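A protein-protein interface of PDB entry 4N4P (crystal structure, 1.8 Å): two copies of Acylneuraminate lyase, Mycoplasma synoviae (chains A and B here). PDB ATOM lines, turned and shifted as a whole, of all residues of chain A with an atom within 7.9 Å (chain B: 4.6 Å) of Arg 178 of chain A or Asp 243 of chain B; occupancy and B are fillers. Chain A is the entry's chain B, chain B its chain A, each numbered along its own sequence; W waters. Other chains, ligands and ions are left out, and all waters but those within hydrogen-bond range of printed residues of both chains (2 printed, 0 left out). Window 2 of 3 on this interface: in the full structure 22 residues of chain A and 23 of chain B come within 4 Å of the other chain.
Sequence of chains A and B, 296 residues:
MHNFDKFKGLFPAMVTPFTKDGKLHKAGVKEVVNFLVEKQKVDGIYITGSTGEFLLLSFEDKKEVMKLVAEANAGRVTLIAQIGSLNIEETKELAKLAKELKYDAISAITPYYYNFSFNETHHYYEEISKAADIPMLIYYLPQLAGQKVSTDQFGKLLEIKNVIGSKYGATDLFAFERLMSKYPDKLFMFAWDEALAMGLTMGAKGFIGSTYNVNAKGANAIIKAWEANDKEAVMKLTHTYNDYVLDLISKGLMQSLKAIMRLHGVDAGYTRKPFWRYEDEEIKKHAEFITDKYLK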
ATOM      1  N   SER A 150     -11.731  11.889 -21.582  1.00  0.00           N
ATOM      2  CA  SER A 150     -13.063  11.732 -21.018  1.00  0.00           C
ATOM      3  C   SER A 150     -13.846  10.666 -21.804  1.00  0.00           C
ATOM      4  O   SER A 150     -13.433  10.248 -22.896  1.00  0.00           O
ATOM      5  CB  SER A 150     -13.790  13.067 -21.095  1.00  0.00           C
ATOM      6  OG  SER A 150     -13.931  13.435 -22.457  1.00  0.00           O
ATOM      7  N   THR A 151     -14.982  10.246 -21.241  1.00  0.00           N
ATOM      8  CA  THR A 151     -15.891   9.299 -21.900  1.00  0.00           C
ATOM      9  C   THR A 151     -16.157   9.775 -23.326  1.00  0.00           C
ATOM     10  O   THR A 151     -16.113   8.988 -24.275  1.00  0.00           O
ATOM     11  CB  THR A 151     -17.238   9.163 -21.120  1.00  0.00           C
ATOM     12  OG1 THR A 151     -16.975   8.939 -19.730  1.00  0.00           O
ATOM     13  CG2 THR A 151     -18.069   8.002 -21.653  1.00  0.00           C
ATOM     14  N   ASP A 152     -16.412  11.079 -23.459  1.00  0.00           N
ATOM     15  CA  ASP A 152     -16.708  11.691 -24.756  1.00  0.00           C
ATOM     16  C   ASP A 152     -15.544  11.632 -25.745  1.00  0.00           C
ATOM     17  O   ASP A 152     -15.734  11.255 -26.901  1.00  0.00           O
ATOM     18  CB  ASP A 152     -17.208  13.130 -24.584  1.00  0.00           C
ATOM     19  CG  ASP A 152     -18.611  13.193 -24.019  1.00  0.00           C
ATOM     20  OD1 ASP A 152     -19.357  12.191 -24.133  1.00  0.00           O
ATOM     21  OD2 ASP A 152     -18.978  14.248 -23.449  1.00  0.00           O
ATOM     22  N   TYR A 168     -11.495  -3.378 -22.633  1.00  0.00           N
ATOM     23  CA  TYR A 168     -11.465  -2.538 -21.429  1.00  0.00           C
ATOM     24  C   TYR A 168     -10.705  -3.232 -20.307  1.00  0.00           C
ATOM     25  O   TYR A 168     -11.259  -4.091 -19.645  1.00  0.00           O
ATOM     26  CB  TYR A 168     -12.885  -2.182 -20.962  1.00  0.00           C
ATOM     27  CG  TYR A 168     -12.824  -1.107 -19.886  1.00  0.00           C
ATOM     28  CD1 TYR A 168     -12.665  -1.440 -18.540  1.00  0.00           C
ATOM     29  CD2 TYR A 168     -12.837   0.248 -20.239  1.00  0.00           C
ATOM     30  CE1 TYR A 168     -12.555  -0.443 -17.549  1.00  0.00           C
ATOM     31  CE2 TYR A 168     -12.747   1.248 -19.272  1.00  0.00           C
ATOM     32  CZ  TYR A 168     -12.604   0.889 -17.930  1.00  0.00           C
ATOM     33  OH  TYR A 168     -12.474   1.873 -16.988  1.00  0.00           O
ATOM     34  N   ASP A 172     -10.785   0.886 -13.312  1.00  0.00           N
ATOM     35  CA  ASP A 172     -11.748   1.956 -13.054  1.00  0.00           C
ATOM     36  C   ASP A 172     -13.160   1.514 -13.472  1.00  0.00           C
ATOM     37  O   ASP A 172     -13.513   1.547 -14.659  1.00  0.00           O
ATOM     38  CB  ASP A 172     -11.339   3.194 -13.832  1.00  0.00           C
ATOM     39  CG  ASP A 172     -12.234   4.386 -13.564  1.00  0.00           C
ATOM     40  OD1 ASP A 172     -13.337   4.223 -13.007  1.00  0.00           O
ATOM     41  OD2 ASP A 172     -11.804   5.493 -13.906  1.00  0.00           O
ATOM     42  N   LEU A 173     -13.953   1.069 -12.504  1.00  0.00           N
ATOM     43  CA  LEU A 173     -15.267   0.504 -12.827  1.00  0.00           C
ATOM     44  C   LEU A 173     -16.294   1.590 -13.111  1.00  0.00           C
ATOM     45  O   LEU A 173     -17.310   1.353 -13.776  1.00  0.00           O
ATOM     46  CB  LEU A 173     -15.750  -0.447 -11.729  1.00  0.00           C
ATOM     47  CG  LEU A 173     -14.765  -1.621 -11.587  1.00  0.00           C
ATOM     48  CD1 LEU A 173     -14.983  -2.395 -10.300  1.00  0.00           C
ATOM     49  CD2 LEU A 173     -14.827  -2.558 -12.771  1.00  0.00           C
ATOM     50  N   PHE A 174     -16.030   2.789 -12.597  1.00  0.00           N
ATOM     51  CA  PHE A 174     -16.911   3.915 -12.894  1.00  0.00           C
ATOM     52  C   PHE A 174     -16.753   4.329 -14.354  1.00  0.00           C
ATOM     53  O   PHE A 174     -17.738   4.464 -15.077  1.00  0.00           O
ATOM     54  CB  PHE A 174     -16.636   5.093 -11.962  1.00  0.00           C
ATOM     55  CG  PHE A 174     -17.557   6.251 -12.181  1.00  0.00           C
ATOM     56  CD1 PHE A 174     -18.930   6.109 -12.001  1.00  0.00           C
ATOM     57  CD2 PHE A 174     -17.064   7.479 -12.611  1.00  0.00           C
ATOM     58  CE1 PHE A 174     -19.810   7.195 -12.177  1.00  0.00           C
ATOM     59  CE2 PHE A 174     -17.943   8.575 -12.818  1.00  0.00           C
ATOM     60  CZ  PHE A 174     -19.312   8.425 -12.586  1.00  0.00           C
ATOM     61  N   ALA A 175     -15.516   4.479 -14.822  1.00  0.00           N
ATOM     62  CA  ALA A 175     -15.338   4.745 -16.258  1.00  0.00           C
ATOM     63  C   ALA A 175     -16.003   3.680 -17.133  1.00  0.00           C
ATOM     64  O   ALA A 175     -16.539   3.999 -18.189  1.00  0.00           O
ATOM     65  CB  ALA A 175     -13.845   4.887 -16.613  1.00  0.00           C
ATOM     66  N   PHE A 176     -15.970   2.413 -16.708  1.00  0.00           N
ATOM     67  CA  PHE A 176     -16.583   1.330 -17.479  1.00  0.00           C
ATOM     68  C   PHE A 176     -18.098   1.510 -17.531  1.00  0.00           C
ATOM     69  O   PHE A 176     -18.710   1.435 -18.598  1.00  0.00           O
ATOM     70  CB  PHE A 176     -16.282  -0.039 -16.864  1.00  0.00           C
ATOM     71  CG  PHE A 176     -16.956  -1.171 -17.584  1.00  0.00           C
ATOM     72  CD1 PHE A 176     -16.575  -1.505 -18.896  1.00  0.00           C
ATOM     73  CD2 PHE A 176     -17.981  -1.890 -16.967  1.00  0.00           C
ATOM     74  CE1 PHE A 176     -17.214  -2.527 -19.610  1.00  0.00           C
ATOM     75  CE2 PHE A 176     -18.625  -2.940 -17.669  1.00  0.00           C
ATOM     76  CZ  PHE A 176     -18.231  -3.259 -18.981  1.00  0.00           C
ATOM     77  N   GLU A 177     -18.691   1.745 -16.366  1.00  0.00           N
ATOM     78  CA  GLU A 177     -20.125   2.046 -16.294  1.00  0.00           C
ATOM     79  C   GLU A 177     -20.485   3.232 -17.205  1.00  0.00           C
ATOM     80  O   GLU A 177     -21.494   3.170 -17.926  1.00  0.00           O
ATOM     81  CB  GLU A 177     -20.543   2.306 -14.844  1.00  0.00           C
ATOM     82  CG  GLU A 177     -22.039   2.631 -14.685  1.00  0.00           C
ATOM     83  CD  GLU A 177     -22.373   4.094 -14.974  1.00  0.00           C
ATOM     84  OE1 GLU A 177     -21.570   4.989 -14.601  1.00  0.00           O
ATOM     85  OE2 GLU A 177     -23.481   4.342 -15.511  1.00  0.00           O
ATOM     86  N   ARG A 178     -19.684   4.294 -17.163  1.00  0.00           N
ATOM     87  CA  ARG A 178     -19.921   5.467 -18.018  1.00  0.00           C
ATOM     88  C   ARG A 178     -19.878   5.121 -19.516  1.00  0.00           C
ATOM     89  O   ARG A 178     -20.682   5.624 -20.298  1.00  0.00           O
ATOM     90  CB  ARG A 178     -18.932   6.590 -17.693  1.00  0.00           C
ATOM     91  CG  ARG A 178     -19.073   7.165 -16.267  1.00  0.00           C
ATOM     92  CD  ARG A 178     -20.336   8.130 -16.194  1.00  0.00           C
ATOM     93  NE  ARG A 178     -21.586   7.378 -16.017  1.00  0.00           N
ATOM     94  CZ  ARG A 178     -22.810   7.904 -16.153  1.00  0.00           C
ATOM     95  NH1 ARG A 178     -23.880   7.145 -15.979  1.00  0.00           N
ATOM     96  NH2 ARG A 178     -22.961   9.197 -16.453  1.00  0.00           N
ATOM     97  N   LEU A 179     -18.919   4.283 -19.927  1.00  0.00           N
ATOM     98  CA  LEU A 179     -18.837   3.862 -21.332  1.00  0.00           C
ATOM     99  C   LEU A 179     -20.033   3.023 -21.727  1.00  0.00           C
ATOM    100  O   LEU A 179     -20.583   3.195 -22.817  1.00  0.00           O
ATOM    101  CB  LEU A 179     -17.546   3.061 -21.602  1.00  0.00           C
ATOM    102  CG  LEU A 179     -16.240   3.841 -21.546  1.00  0.00           C
ATOM    103  CD1 LEU A 179     -15.029   2.876 -21.579  1.00  0.00           C
ATOM    104  CD2 LEU A 179     -16.175   4.822 -22.721  1.00  0.00           C
ATOM    105  N   MET A 180     -20.432   2.089 -20.866  1.00  0.00           N
ATOM    106  CA  MET A 180     -21.635   1.281 -21.145  1.00  0.00           C
ATOM    107  C   MET A 180     -22.907   2.148 -21.292  1.00  0.00           C
ATOM    108  O   MET A 180     -23.769   1.812 -22.099  1.00  0.00           O
ATOM    109  CB  MET A 180     -21.871   0.231 -20.078  1.00  0.00           C
ATOM    110  CG  MET A 180     -20.788  -0.846 -20.001  1.00  0.00           C
ATOM    111  SD  MET A 180     -20.587  -1.829 -21.508  1.00  0.00           S
ATOM    112  CE  MET A 180     -22.109  -2.775 -21.511  1.00  0.00           C
ATOM    113  N   SER A 181     -23.011   3.229 -20.524  1.00  0.00           N
ATOM    114  CA  SER A 181     -24.152   4.142 -20.618  1.00  0.00           C
ATOM    115  C   SER A 181     -24.137   4.907 -21.920  1.00  0.00           C
ATOM    116  O   SER A 181     -25.153   5.010 -22.610  1.00  0.00           O
ATOM    117  CB  SER A 181     -24.119   5.137 -19.472  1.00  0.00           C
ATOM    118  OG  SER A 181     -25.337   5.872 -19.449  1.00  0.00           O
ATOM    119  N   LYS A 182     -22.964   5.396 -22.270  1.00  0.00           N
ATOM    120  CA  LYS A 182     -22.812   6.320 -23.381  1.00  0.00           C
ATOM    121  C   LYS A 182     -22.742   5.658 -24.751  1.00  0.00           C
ATOM    122  O   LYS A 182     -23.209   6.256 -25.734  1.00  0.00           O
ATOM    123  CB  LYS A 182     -21.573   7.173 -23.129  1.00  0.00           C
ATOM    124  CG  LYS A 182     -21.347   8.308 -24.102  1.00  0.00           C
ATOM    125  CD  LYS A 182     -22.447   9.375 -24.060  1.00  0.00           C
ATOM    126  CE  LYS A 182     -22.209  10.423 -25.169  1.00  0.00           C
ATOM    127  NZ  LYS A 182     -20.734  10.577 -25.472  1.00  0.00           N
ATOM    128  N   TYR A 183     -22.184   4.441 -24.815  1.00  0.00           N
ATOM    129  CA  TYR A 183     -21.964   3.741 -26.094  1.00  0.00           C
ATOM    130  C   TYR A 183     -22.631   2.378 -26.112  1.00  0.00           C
ATOM    131  O   TYR A 183     -21.946   1.355 -26.216  1.00  0.00           O
ATOM    132  CB  TYR A 183     -20.453   3.624 -26.398  1.00  0.00           C
ATOM    133  CG  TYR A 183     -19.771   4.971 -26.363  1.00  0.00           C
ATOM    134  CD1 TYR A 183     -19.947   5.891 -27.402  1.00  0.00           C
ATOM    135  CD2 TYR A 183     -18.986   5.334 -25.278  1.00  0.00           C
ATOM    136  CE1 TYR A 183     -19.355   7.129 -27.354  1.00  0.00           C
ATOM    137  CE2 TYR A 183     -18.386   6.572 -25.214  1.00  0.00           C
ATOM    138  CZ  TYR A 183     -18.584   7.467 -26.255  1.00  0.00           C
ATOM    139  OH  TYR A 183     -17.985   8.692 -26.184  1.00  0.00           O
ATOM    140  N   PRO A 184     -23.983   2.348 -26.028  1.00  0.00           N
ATOM    141  CA  PRO A 184     -24.683   1.068 -25.963  1.00  0.00           C
ATOM    142  C   PRO A 184     -24.557   0.293 -27.275  1.00  0.00           C
ATOM    143  O   PRO A 184     -24.802  -0.917 -27.287  1.00  0.00           O
ATOM    144  CB  PRO A 184     -26.158   1.481 -25.721  1.00  0.00           C
ATOM    145  CG  PRO A 184     -26.264   2.803 -26.328  1.00  0.00           C
ATOM    146  CD  PRO A 184     -24.934   3.478 -26.034  1.00  0.00           C
ATOM    147  N   PHE A 188     -17.869  -3.811 -25.566  1.00  0.00           N
ATOM    148  CA  PHE A 188     -16.756  -3.658 -24.622  1.00  0.00           C
ATOM    149  C   PHE A 188     -16.405  -5.007 -24.087  1.00  0.00           C
ATOM    150  O   PHE A 188     -17.202  -5.639 -23.398  1.00  0.00           O
ATOM    151  CB  PHE A 188     -17.076  -2.655 -23.497  1.00  0.00           C
ATOM    152  CG  PHE A 188     -17.287  -1.269 -24.012  1.00  0.00           C
ATOM    153  CD1 PHE A 188     -16.195  -0.433 -24.258  1.00  0.00           C
ATOM    154  CD2 PHE A 188     -18.560  -0.836 -24.377  1.00  0.00           C
ATOM    155  CE1 PHE A 188     -16.381   0.872 -24.778  1.00  0.00           C
ATOM    156  CE2 PHE A 188     -18.749   0.451 -24.901  1.00  0.00           C
ATOM    157  CZ  PHE A 188     -17.643   1.312 -25.098  1.00  0.00           C
ATOM    158  N   MET A 202     -22.613  -4.597 -14.759  1.00  0.00           N
ATOM    159  CA  MET A 202     -22.816  -3.399 -15.590  1.00  0.00           C
ATOM    160  C   MET A 202     -22.940  -3.688 -17.091  1.00  0.00           C
ATOM    161  O   MET A 202     -22.846  -2.763 -17.914  1.00  0.00           O
ATOM    162  CB  MET A 202     -21.788  -2.286 -15.274  1.00  0.00           C
ATOM    163  CG  MET A 202     -22.313  -1.159 -14.257  1.00  0.00           C
ATOM    164  SD  MET A 202     -24.074  -0.708 -14.548  1.00  0.00           S
ATOM    165  CE  MET A 202     -24.762  -1.495 -13.069  1.00  0.00           C
ATOM    166  N   HIS B 239     -27.196   3.626 -14.628  1.00  0.00           N
ATOM    167  CA  HIS B 239     -26.788   4.689 -15.579  1.00  0.00           C
ATOM    168  C   HIS B 239     -27.511   5.982 -15.254  1.00  0.00           C
ATOM    169  O   HIS B 239     -26.893   7.044 -15.210  1.00  0.00           O
ATOM    170  CB  HIS B 239     -27.037   4.252 -17.032  1.00  0.00           C
ATOM    171  CG  HIS B 239     -26.239   3.040 -17.424  1.00  0.00           C
ATOM    172  ND1 HIS B 239     -24.950   2.827 -16.985  1.00  0.00           N
ATOM    173  CD2 HIS B 239     -26.550   1.977 -18.209  1.00  0.00           C
ATOM    174  CE1 HIS B 239     -24.498   1.684 -17.477  1.00  0.00           C
ATOM    175  NE2 HIS B 239     -25.444   1.153 -18.234  1.00  0.00           N
ATOM    176  N   THR B 240     -28.808   5.875 -14.952  1.00  0.00           N
ATOM    177  CA  THR B 240     -29.584   7.044 -14.551  1.00  0.00           C
ATOM    178  C   THR B 240     -29.060   7.655 -13.257  1.00  0.00           C
ATOM    179  O   THR B 240     -28.845   8.858 -13.186  1.00  0.00           O
ATOM    180  CB  THR B 240     -31.073   6.713 -14.420  1.00  0.00           C
ATOM    181  OG1 THR B 240     -31.530   6.280 -15.706  1.00  0.00           O
ATOM    182  CG2 THR B 240     -31.877   7.972 -14.004  1.00  0.00           C
ATOM    183  N   TYR B 241     -28.859   6.818 -12.240  1.00  0.00           N
ATOM    184  CA  TYR B 241     -28.347   7.295 -10.954  1.00  0.00           C
ATOM    185  C   TYR B 241     -26.997   7.989 -11.108  1.00  0.00           C
ATOM    186  O   TYR B 241     -26.726   9.029 -10.513  1.00  0.00           O
ATOM    187  CB  TYR B 241     -28.251   6.136  -9.937  1.00  0.00           C
ATOM    188  CG  TYR B 241     -28.246   6.656  -8.523  1.00  0.00           C
ATOM    189  CD1 TYR B 241     -29.448   6.992  -7.881  1.00  0.00           C
ATOM    190  CD2 TYR B 241     -27.034   6.907  -7.864  1.00  0.00           C
ATOM    191  CE1 TYR B 241     -29.447   7.527  -6.603  1.00  0.00           C
ATOM    192  CE2 TYR B 241     -27.016   7.449  -6.574  1.00  0.00           C
ATOM    193  CZ  TYR B 241     -28.240   7.749  -5.954  1.00  0.00           C
ATOM    194  OH  TYR B 241     -28.257   8.272  -4.696  1.00  0.00           O
ATOM    195  N   ASN B 242     -26.127   7.416 -11.910  1.00  0.00           N
ATOM    196  CA  ASN B 242     -24.789   8.014 -12.018  1.00  0.00           C
ATOM    197  C   ASN B 242     -24.817   9.270 -12.864  1.00  0.00           C
ATOM    198  O   ASN B 242     -24.038  10.170 -12.630  1.00  0.00           O
ATOM    199  CB  ASN B 242     -23.790   6.985 -12.538  1.00  0.00           C
ATOM    200  CG  ASN B 242     -23.452   5.930 -11.451  1.00  0.00           C
ATOM    201  OD1 ASN B 242     -24.010   5.980 -10.351  1.00  0.00           O
ATOM    202  ND2 ASN B 242     -22.540   5.008 -11.754  1.00  0.00           N
ATOM    203  N   ASP B 243     -25.769   9.340 -13.798  1.00  0.00           N
ATOM    204  CA  ASP B 243     -26.028  10.599 -14.515  1.00  0.00           C
ATOM    205  C   ASP B 243     -26.393  11.652 -13.474  1.00  0.00           C
ATOM    206  O   ASP B 243     -25.880  12.779 -13.497  1.00  0.00           O
ATOM    207  CB  ASP B 243     -27.192  10.456 -15.508  1.00  0.00           C
ATOM    208  CG  ASP B 243     -26.813   9.736 -16.786  1.00  0.00           C
ATOM    209  OD1 ASP B 243     -25.625   9.468 -17.045  1.00  0.00           O
ATOM    210  OD2 ASP B 243     -27.740   9.448 -17.543  1.00  0.00           O
ATOM    211  N   TYR B 244     -27.277  11.262 -12.565  1.00  0.00           N
ATOM    212  CA  TYR B 244     -27.748  12.139 -11.483  1.00  0.00           C
ATOM    213  C   TYR B 244     -26.598  12.614 -10.617  1.00  0.00           C
ATOM    214  O   TYR B 244     -26.480  13.804 -10.342  1.00  0.00           O
ATOM    215  CB  TYR B 244     -28.813  11.428 -10.637  1.00  0.00           C
ATOM    216  CG  TYR B 244     -28.854  11.808  -9.167  1.00  0.00           C
ATOM    217  CD1 TYR B 244     -29.301  13.078  -8.751  1.00  0.00           C
ATOM    218  CD2 TYR B 244     -28.460  10.872  -8.174  1.00  0.00           C
ATOM    219  CE1 TYR B 244     -29.339  13.421  -7.375  1.00  0.00           C
ATOM    220  CE2 TYR B 244     -28.519  11.186  -6.814  1.00  0.00           C
ATOM    221  CZ  TYR B 244     -28.943  12.462  -6.418  1.00  0.00           C
ATOM    222  OH  TYR B 244     -28.989  12.781  -5.076  1.00  0.00           O
ATOM    223  N   VAL B 245     -25.746  11.685 -10.187  1.00  0.00           N
ATOM    224  CA  VAL B 245     -24.629  12.076  -9.322  1.00  0.00           C
ATOM    225  C   VAL B 245     -23.731  13.101 -10.010  1.00  0.00           C
ATOM    226  O   VAL B 245     -23.416  14.134  -9.423  1.00  0.00           O
ATOM    227  CB  VAL B 245     -23.804  10.867  -8.844  1.00  0.00           C
ATOM    228  CG1 VAL B 245     -22.665  11.345  -7.929  1.00  0.00           C
ATOM    229  CG2 VAL B 245     -24.722   9.848  -8.079  1.00  0.00           C
ATOM    230  N   LEU B 246     -23.333  12.832 -11.256  1.00  0.00           N
ATOM    231  CA  LEU B 246     -22.480  13.759 -11.995  1.00  0.00           C
ATOM    232  C   LEU B 246     -23.164  15.136 -12.217  1.00  0.00           C
ATOM    233  O   LEU B 246     -22.515  16.204 -12.097  1.00  0.00           O
ATOM    234  CB  LEU B 246     -22.061  13.134 -13.337  1.00  0.00           C
ATOM    235  CG  LEU B 246     -21.088  11.964 -13.134  1.00  0.00           C
ATOM    236  CD1 LEU B 246     -20.641  11.349 -14.461  1.00  0.00           C
ATOM    237  CD2 LEU B 246     -19.886  12.408 -12.306  1.00  0.00           C
ATOM    238  N   ASP B 247     -24.461  15.106 -12.507  1.00  0.00           N
ATOM    239  CA  ASP B 247     -25.216  16.361 -12.689  1.00  0.00           C
ATOM    240  C   ASP B 247     -25.263  17.107 -11.360  1.00  0.00           C
ATOM    241  O   ASP B 247     -25.058  18.332 -11.310  1.00  0.00           O
ATOM    242  CB  ASP B 247     -26.646  16.095 -13.232  1.00  0.00           C
ATOM    243  CG  ASP B 247     -26.699  15.995 -14.746  1.00  0.00           C
ATOM    244  OD1 ASP B 247     -25.753  16.412 -15.432  1.00  0.00           O
ATOM    245  OD2 ASP B 247     -27.736  15.559 -15.262  1.00  0.00           O
ATOM    246  N   TYR B 294     -34.544  14.144 -12.175  1.00  0.00           N
ATOM    247  CA  TYR B 294     -34.298  12.854 -11.484  1.00  0.00           C
ATOM    248  C   TYR B 294     -35.253  12.500 -10.367  1.00  0.00           C
ATOM    249  O   TYR B 294     -35.422  11.310 -10.074  1.00  0.00           O
ATOM    250  CB  TYR B 294     -32.875  12.833 -10.922  1.00  0.00           C
ATOM    251  CG  TYR B 294     -31.812  12.937 -11.977  1.00  0.00           C
ATOM    252  CD1 TYR B 294     -31.575  11.866 -12.866  1.00  0.00           C
ATOM    253  CD2 TYR B 294     -31.059  14.105 -12.106  1.00  0.00           C
ATOM    254  CE1 TYR B 294     -30.604  11.957 -13.836  1.00  0.00           C
ATOM    255  CE2 TYR B 294     -30.065  14.217 -13.078  1.00  0.00           C
ATOM    256  CZ  TYR B 294     -29.847  13.129 -13.936  1.00  0.00           C
ATOM    257  OH  TYR B 294     -28.885  13.216 -14.909  1.00  0.00           O
HETATM  258  O   HOH W   1     -24.730   8.414 -19.412  1.00  0.00           O
HETATM  259  O   HOH W   2     -25.050  -1.412 -19.158  1.00  0.00           O
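Water W1 lies within hydrogen-bond range of the side-chain hydroxyl of Ser 181 of chain A (2.6 Å) and the side-chain carboxylate of Asp 243 of chain B (2.7 Å). Water W2 bridges NE2 of His 239 of chain B (2.8 Å) and O of Met 202 of chain A (2.9 Å).
Hydrophobic or aromatic side chains of chain A that line the printed part of chain B: Phe 174, Met 180 and Met 202. Along chain A the printed residues that touch a printed residue of chain B span positions 174 to 202. Of the 10 printed residues of chain B, 4 touch a printed residue of chain A. Among the printed residues, 11 pairs touch across the chains. Among the printed residues, Asp or Glu carboxylates within 4 Å of a Lys or Arg side-chain nitrogen of the other chain: Arg 178 of chain A with Asp 243 of chain B (2.7 Å).
ND1 of His 239 of chain B lies within hydrogen-bond range of OE2 of Glu 177 of chain A (2.6 Å). The backbone carbonyl oxygen (O) of His 239 of chain B is in hydrogen-bond range of the guanidinium group (NH1) of Arg 178 of chain A. The side-chain amide nitrogen (ND2) of Asn 242 of chain B lies within hydrogen-bond range of the side-chain carboxylate (OE1) of Glu 177 of chain A, at 3.0 Å. The guanidinium group (NH2) of Arg 178 of chain A lies within salt-bridge range of the side-chain carboxylate (OD1) of Asp 243 of chain B.
The side-chain hydroxyl (OH) of Tyr 294 of chain B lies close to the backbone carbonyl oxygen (O) of Asp 243 of chain B (3.3 Å). The backbone NH of Phe 174 of chain A sits at hydrogen-bond distance from the side-chain carboxylate of Asp 172 of chain A (3.1 Å). The guanidinium group of Arg 178 of chain A lies within salt-bridge range of the side-chain carboxylate of Glu 177 of chain A, at 2.8 Å.
Among the printed residues, merely in contact across the chains: Ser 181 of chain A with His 239 of chain B (3.4 Å), Arg 178 of chain A with Asn 242 of chain B (3.4 Å), Phe 174 of chain A with Asn 242 of chain B (3.5 Å), Arg 178 of chain A with Leu 246 of chain B (3.7 Å), Phe 174 of chain A with Leu 246 of chain B (3.7 Å), Met 202 of chain A with His 239 of chain B (3.8 Å) and Met 180 of chain A with His 239 of chain B (3.97 Å).
Asp 152 of chain A touches none of the printed residues of chain B. Arg 178 of chain A touches just these residues of chain B: His 239, Asn 242, Asp 243 and Leu 246. Of the printed residues of chain B, Met 180 of chain A touches His 239 (3.97 Å). Of the printed residues of chain B, Ser 181 of chain A touches His 239 (3.4 Å). Tyr 241 of chain B touches none of the printed residues of chain A. Of the printed residues of chain A, Asn 242 of chain B touches Phe 174, Glu 177 and Arg 178. Asp 243 of chain B touches just one residue of chain A: Arg 178. Printed residues of chain A within 4 Å of Leu 246 of chain B: Phe 174 and Arg 178. The nearest residue of chain A that does not touch Asp 243 of chain B is Ser 181 of chain A (4.3 Å). The nearest printed residue of chain A that does not touch Asn 242 of chain B is Met 202 of chain A (6.5 Å).
No position is printed for both chains. Of the 11 pairs that touch across the chains among the printed residues, none has its exchanged pair printed and touching as well.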
